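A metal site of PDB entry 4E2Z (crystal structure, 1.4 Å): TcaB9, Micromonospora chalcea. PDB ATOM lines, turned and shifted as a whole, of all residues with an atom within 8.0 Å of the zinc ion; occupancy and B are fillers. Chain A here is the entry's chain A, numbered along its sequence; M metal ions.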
ATOM      1  N   ALA A  14     -10.808  16.368 -18.312  1.00  0.00           N
ATOM      2  CA  ALA A  14     -10.758  15.162 -19.146  1.00  0.00           C
ATOM      3  C   ALA A  14     -11.614  14.062 -18.504  1.00  0.00           C
ATOM      4  O   ALA A  14     -11.526  13.828 -17.295  1.00  0.00           O
ATOM      5  CB  ALA A  14      -9.316  14.654 -19.282  1.00  0.00           C
ATOM      6  N   CYS A  15     -12.416  13.366 -19.306  1.00  0.00           N
ATOM      7  CA  CYS A  15     -13.083  12.126 -18.890  1.00  0.00           C
ATOM      8  C   CYS A  15     -12.176  11.110 -18.202  1.00  0.00           C
ATOM      9  O   CYS A  15     -11.086  10.831 -18.716  1.00  0.00           O
ATOM     10  CB  CYS A  15     -13.853  11.500 -20.064  1.00  0.00           C
ATOM     11  SG  CYS A  15     -14.705   9.964 -19.703  1.00  0.00           S
ATOM     12  N   ARG A  16     -12.617  10.567 -17.067  1.00  0.00           N
ATOM     13  CA  ARG A  16     -11.862   9.550 -16.345  1.00  0.00           C
ATOM     14  C   ARG A  16     -11.909   8.154 -16.956  1.00  0.00           C
ATOM     15  O   ARG A  16     -11.066   7.309 -16.638  1.00  0.00           O
ATOM     16  CB  ARG A  16     -12.291   9.473 -14.870  1.00  0.00           C
ATOM     17  CG  ARG A  16     -11.711  10.592 -14.043  1.00  0.00           C
ATOM     18  CD  ARG A  16     -10.156  10.452 -14.005  1.00  0.00           C
ATOM     19  NE  ARG A  16      -9.673  10.487 -12.628  1.00  0.00           N
ATOM     20  CZ  ARG A  16      -8.762   9.684 -12.071  1.00  0.00           C
ATOM     21  NH1 ARG A  16      -8.465   9.908 -10.798  1.00  0.00           N
ATOM     22  NH2 ARG A  16      -8.145   8.706 -12.719  1.00  0.00           N
ATOM     23  N   VAL A  17     -12.857   7.912 -17.850  1.00  0.00           N
ATOM     24  CA  VAL A  17     -12.901   6.616 -18.528  1.00  0.00           C
ATOM     25  C   VAL A  17     -12.037   6.682 -19.796  1.00  0.00           C
ATOM     26  O   VAL A  17     -11.214   5.793 -20.010  1.00  0.00           O
ATOM     27  CB  VAL A  17     -14.347   6.156 -18.836  1.00  0.00           C
ATOM     28  CG1 VAL A  17     -14.348   4.868 -19.660  1.00  0.00           C
ATOM     29  CG2 VAL A  17     -15.155   5.990 -17.532  1.00  0.00           C
ATOM     30  N   CYS A  18     -12.173   7.719 -20.624  1.00  0.00           N
ATOM     31  CA  CYS A  18     -11.669   7.689 -22.009  1.00  0.00           C
ATOM     32  C   CYS A  18     -10.765   8.872 -22.381  1.00  0.00           C
ATOM     33  O   CYS A  18     -10.196   8.891 -23.472  1.00  0.00           O
ATOM     34  CB  CYS A  18     -12.792   7.514 -23.042  1.00  0.00           C
ATOM     35  SG  CYS A  18     -13.653   9.070 -23.459  1.00  0.00           S
ATOM     36  N   GLY A  19     -10.613   9.864 -21.506  1.00  0.00           N
ATOM     37  CA  GLY A  19      -9.845  11.078 -21.824  1.00  0.00           C
ATOM     38  C   GLY A  19     -10.542  12.103 -22.712  1.00  0.00           C
ATOM     39  O   GLY A  19      -9.995  13.192 -22.943  1.00  0.00           O
ATOM     40  N   GLY A  20     -11.757  11.833 -23.198  1.00  0.00           N
ATOM     41  CA  GLY A  20     -12.559  12.780 -23.974  1.00  0.00           C
ATOM     42  C   GLY A  20     -12.834  14.056 -23.199  1.00  0.00           C
ATOM     43  O   GLY A  20     -12.514  14.152 -22.013  1.00  0.00           O
ATOM     44  N   GLY A  21     -13.465  15.039 -23.836  1.00  0.00           N
ATOM     45  CA  GLY A  21     -13.810  16.283 -23.153  1.00  0.00           C
ATOM     46  C   GLY A  21     -15.137  16.236 -22.420  1.00  0.00           C
ATOM     47  O   GLY A  21     -16.117  15.699 -22.957  1.00  0.00           O
ATOM     48  N   VAL A  22     -15.165  16.792 -21.202  1.00  0.00           N
ATOM     49  CA  VAL A  22     -16.411  16.753 -20.418  1.00  0.00           C
ATOM     50  C   VAL A  22     -17.117  18.097 -20.503  1.00  0.00           C
ATOM     51  O   VAL A  22     -16.479  19.098 -20.181  1.00  0.00           O
ATOM     52  CB  VAL A  22     -16.206  16.334 -18.936  1.00  0.00           C
ATOM     53  CG1 VAL A  22     -17.423  16.502 -18.038  1.00  0.00           C
ATOM     54  CG2 VAL A  22     -15.629  14.917 -18.819  1.00  0.00           C
ATOM     55  N   ARG A  55     -20.823  15.695 -18.958  1.00  0.00           N
ATOM     56  CA  ARG A  55     -21.015  14.480 -19.765  1.00  0.00           C
ATOM     57  C   ARG A  55     -19.812  14.472 -20.709  1.00  0.00           C
ATOM     58  O   ARG A  55     -19.555  15.482 -21.413  1.00  0.00           O
ATOM     59  CB  ARG A  55     -22.361  14.479 -20.517  1.00  0.00           C
ATOM     60  CG  ARG A  55     -22.544  13.130 -21.212  1.00  0.00           C
ATOM     61  CD  ARG A  55     -23.405  13.161 -22.472  1.00  0.00           C
ATOM     62  NE  ARG A  55     -22.685  13.773 -23.578  1.00  0.00           N
ATOM     63  CZ  ARG A  55     -23.250  14.104 -24.736  1.00  0.00           C
ATOM     64  NH1 ARG A  55     -22.455  14.686 -25.630  1.00  0.00           N
ATOM     65  NH2 ARG A  55     -24.527  13.879 -24.958  1.00  0.00           N
ATOM     66  N   CYS A  56     -19.100  13.345 -20.769  1.00  0.00           N
ATOM     67  CA  CYS A  56     -18.045  13.131 -21.763  1.00  0.00           C
ATOM     68  C   CYS A  56     -18.615  13.232 -23.179  1.00  0.00           C
ATOM     69  O   CYS A  56     -19.667  12.663 -23.493  1.00  0.00           O
ATOM     70  CB  CYS A  56     -17.346  11.782 -21.560  1.00  0.00           C
ATOM     71  SG  CYS A  56     -16.046  11.499 -22.807  1.00  0.00           S
ATOM     72  N   ASP A  57     -17.854  13.931 -24.031  1.00  0.00           N
ATOM     73  CA  ASP A  57     -18.115  14.109 -25.462  1.00  0.00           C
ATOM     74  C   ASP A  57     -18.020  12.806 -26.255  1.00  0.00           C
ATOM     75  O   ASP A  57     -18.660  12.671 -27.297  1.00  0.00           O
ATOM     76  CB  ASP A  57     -17.020  15.000 -26.046  1.00  0.00           C
ATOM     77  CG  ASP A  57     -17.362  16.459 -25.895  1.00  0.00           C
ATOM     78  OD1 ASP A  57     -18.568  16.672 -25.630  1.00  0.00           O
ATOM     79  OD2 ASP A  57     -16.465  17.321 -26.018  1.00  0.00           O
ATOM     80  N   SER A  58     -17.220  11.855 -25.782  1.00  0.00           N
ATOM     81  CA  SER A  58     -16.836  10.684 -26.555  1.00  0.00           C
ATOM     82  C   SER A  58     -17.544   9.419 -26.088  1.00  0.00           C
ATOM     83  O   SER A  58     -17.983   8.646 -26.945  1.00  0.00           O
ATOM     84  CB  SER A  58     -15.317  10.495 -26.486  1.00  0.00           C
ATOM     85  OG  SER A  58     -14.715  11.646 -27.056  1.00  0.00           O
ATOM     86  N   CYS A  59     -17.670   9.149 -24.793  1.00  0.00           N
ATOM     87  CA  CYS A  59     -18.218   7.887 -24.312  1.00  0.00           C
ATOM     88  C   CYS A  59     -19.547   8.007 -23.544  1.00  0.00           C
ATOM     89  O   CYS A  59     -20.083   7.010 -23.057  1.00  0.00           O
ATOM     90  CB  CYS A  59     -17.192   7.186 -23.420  1.00  0.00           C
ATOM     91  SG  CYS A  59     -17.032   7.934 -21.749  1.00  0.00           S
ATOM     92  N   GLU A  60     -20.053   9.233 -23.454  1.00  0.00           N
ATOM     93  CA  GLU A  60     -21.313   9.519 -22.786  1.00  0.00           C
ATOM     94  C   GLU A  60     -21.378   9.326 -21.274  1.00  0.00           C
ATOM     95  O   GLU A  60     -22.466   9.419 -20.702  1.00  0.00           O
ATOM     96  CB  GLU A  60     -22.554   8.936 -23.478  1.00  0.00           C
ATOM     97  CG  GLU A  60     -22.691   9.573 -24.879  1.00  0.00           C
ATOM     98  CD  GLU A  60     -23.836   8.926 -25.629  1.00  0.00           C
ATOM     99  OE1 GLU A  60     -24.955   9.461 -25.512  1.00  0.00           O
ATOM    100  OE2 GLU A  60     -23.597   7.883 -26.274  1.00  0.00           O
ATOM    101  N   MET A  61     -20.233   9.108 -20.648  1.00  0.00           N
ATOM    102  CA  MET A  61     -20.190   8.990 -19.210  1.00  0.00           C
ATOM    103  C   MET A  61     -20.488  10.324 -18.520  1.00  0.00           C
ATOM    104  O   MET A  61     -19.840  11.352 -18.739  1.00  0.00           O
ATOM    105  CB  MET A  61     -18.832   8.466 -18.712  1.00  0.00           C
ATOM    106  CG  MET A  61     -18.813   8.207 -17.201  1.00  0.00           C
ATOM    107  SD  MET A  61     -19.887   6.871 -16.655  1.00  0.00           S
ATOM    108  CE  MET A  61     -19.002   5.398 -17.158  1.00  0.00           C
ATOM    109  N   VAL A  62     -21.487  10.284 -17.651  1.00  0.00           N
ATOM    110  CA  VAL A  62     -21.807  11.467 -16.846  1.00  0.00           C
ATOM    111  C   VAL A  62     -20.991  11.351 -15.561  1.00  0.00           C
ATOM    112  O   VAL A  62     -20.930  10.301 -14.896  1.00  0.00           O
ATOM    113  CB  VAL A  62     -23.327  11.419 -16.570  1.00  0.00           C
ATOM    114  CG1 VAL A  62     -23.743  12.463 -15.511  1.00  0.00           C
ATOM    115  CG2 VAL A  62     -24.149  11.634 -17.843  1.00  0.00           C
ATOM    116  N   GLN A  63     -20.338  12.448 -15.184  1.00  0.00           N
ATOM    117  CA  GLN A  63     -19.365  12.426 -14.100  1.00  0.00           C
ATOM    118  C   GLN A  63     -19.196  13.845 -13.531  1.00  0.00           C
ATOM    119  O   GLN A  63     -19.444  14.841 -14.222  1.00  0.00           O
ATOM    120  CB  GLN A  63     -17.973  11.964 -14.520  1.00  0.00           C
ATOM    121  CG  GLN A  63     -17.311  12.854 -15.585  1.00  0.00           C
ATOM    122  CD  GLN A  63     -16.400  12.003 -16.409  1.00  0.00           C
ATOM    123  OE1 GLN A  63     -15.227  11.847 -16.045  1.00  0.00           O
ATOM    124  NE2 GLN A  63     -16.894  11.399 -17.492  1.00  0.00           N
ATOM    125  N   PHE A 229     -19.616   9.086 -10.548  1.00  0.00           N
ATOM    126  CA  PHE A 229     -20.283   8.650 -11.792  1.00  0.00           C
ATOM    127  C   PHE A 229     -21.788   8.483 -11.610  1.00  0.00           C
ATOM    128  O   PHE A 229     -22.285   7.983 -10.594  1.00  0.00           O
ATOM    129  CB  PHE A 229     -19.701   7.302 -12.288  1.00  0.00           C
ATOM    130  CG  PHE A 229     -18.243   7.362 -12.656  1.00  0.00           C
ATOM    131  CD1 PHE A 229     -17.856   8.143 -13.762  1.00  0.00           C
ATOM    132  CD2 PHE A 229     -17.284   6.662 -11.922  1.00  0.00           C
ATOM    133  CE1 PHE A 229     -16.511   8.223 -14.135  1.00  0.00           C
ATOM    134  CE2 PHE A 229     -15.938   6.743 -12.294  1.00  0.00           C
ATOM    135  CZ  PHE A 229     -15.563   7.506 -13.393  1.00  0.00           C
ATOM    136  N   SER A 235     -23.220   4.192 -21.081  1.00  0.00           N
ATOM    137  CA  SER A 235     -21.836   4.445 -20.660  1.00  0.00           C
ATOM    138  C   SER A 235     -21.105   3.243 -20.075  1.00  0.00           C
ATOM    139  O   SER A 235     -19.902   3.110 -20.339  1.00  0.00           O
ATOM    140  CB  SER A 235     -21.763   5.676 -19.739  1.00  0.00           C
ATOM    141  OG  SER A 235     -22.484   5.412 -18.536  1.00  0.00           O
ATOM    142  N   ARG A 242     -14.064  -0.823 -23.700  1.00  0.00           N
ATOM    143  CA  ARG A 242     -12.780  -0.207 -24.001  1.00  0.00           C
ATOM    144  C   ARG A 242     -11.696  -0.897 -23.183  1.00  0.00           C
ATOM    145  O   ARG A 242     -10.514  -0.661 -23.401  1.00  0.00           O
ATOM    146  CB  ARG A 242     -12.805   1.285 -23.626  1.00  0.00           C
ATOM    147  CG  ARG A 242     -13.470   2.240 -24.596  1.00  0.00           C
ATOM    148  CD  ARG A 242     -13.716   3.569 -23.866  1.00  0.00           C
ATOM    149  NE  ARG A 242     -13.933   4.639 -24.837  1.00  0.00           N
ATOM    150  CZ  ARG A 242     -15.096   4.962 -25.398  1.00  0.00           C
ATOM    151  NH1 ARG A 242     -15.132   5.973 -26.257  1.00  0.00           N
ATOM    152  NH2 ARG A 242     -16.194   4.274 -25.093  1.00  0.00           N
HETATM  153 ZN    ZN M   1     -15.359   9.432 -21.887  1.00  0.00          ZN
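The nearest printed residue that does not touch the zinc ion is Gly 20 (4.5 Å).
The backbone NH (N) of Met 61 sits close to the side-chain sulfur (SG) of Cys 59 (3.6 Å). The side-chain sulfur (SG) of Cys 18 sits close to the backbone NH (N) of Gly 20, at 3.4 Å. N of Val 17 lies close to SG of Cys 15, at 3.3 Å. N of Cys 56 sits at hydrogen-bond distance from O of Met 61 (2.9 Å). The backbone NH (N) of Ser 58 sits close to the side-chain sulfur (SG) of Cys 56 (3.2 Å). N of Cys 15 sits at hydrogen-bond distance from O of Gly 20 (2.8 Å). NE2 of Gln 63 sits close to SG of Cys 15, 3.4 Å away.
The zinc ion is bound by SG of Cys 59 (2.2 Å), SG of Cys 15 (2.3 Å), SG of Cys 18 (2.3 Å) and SG of Cys 56 (2.4 Å).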
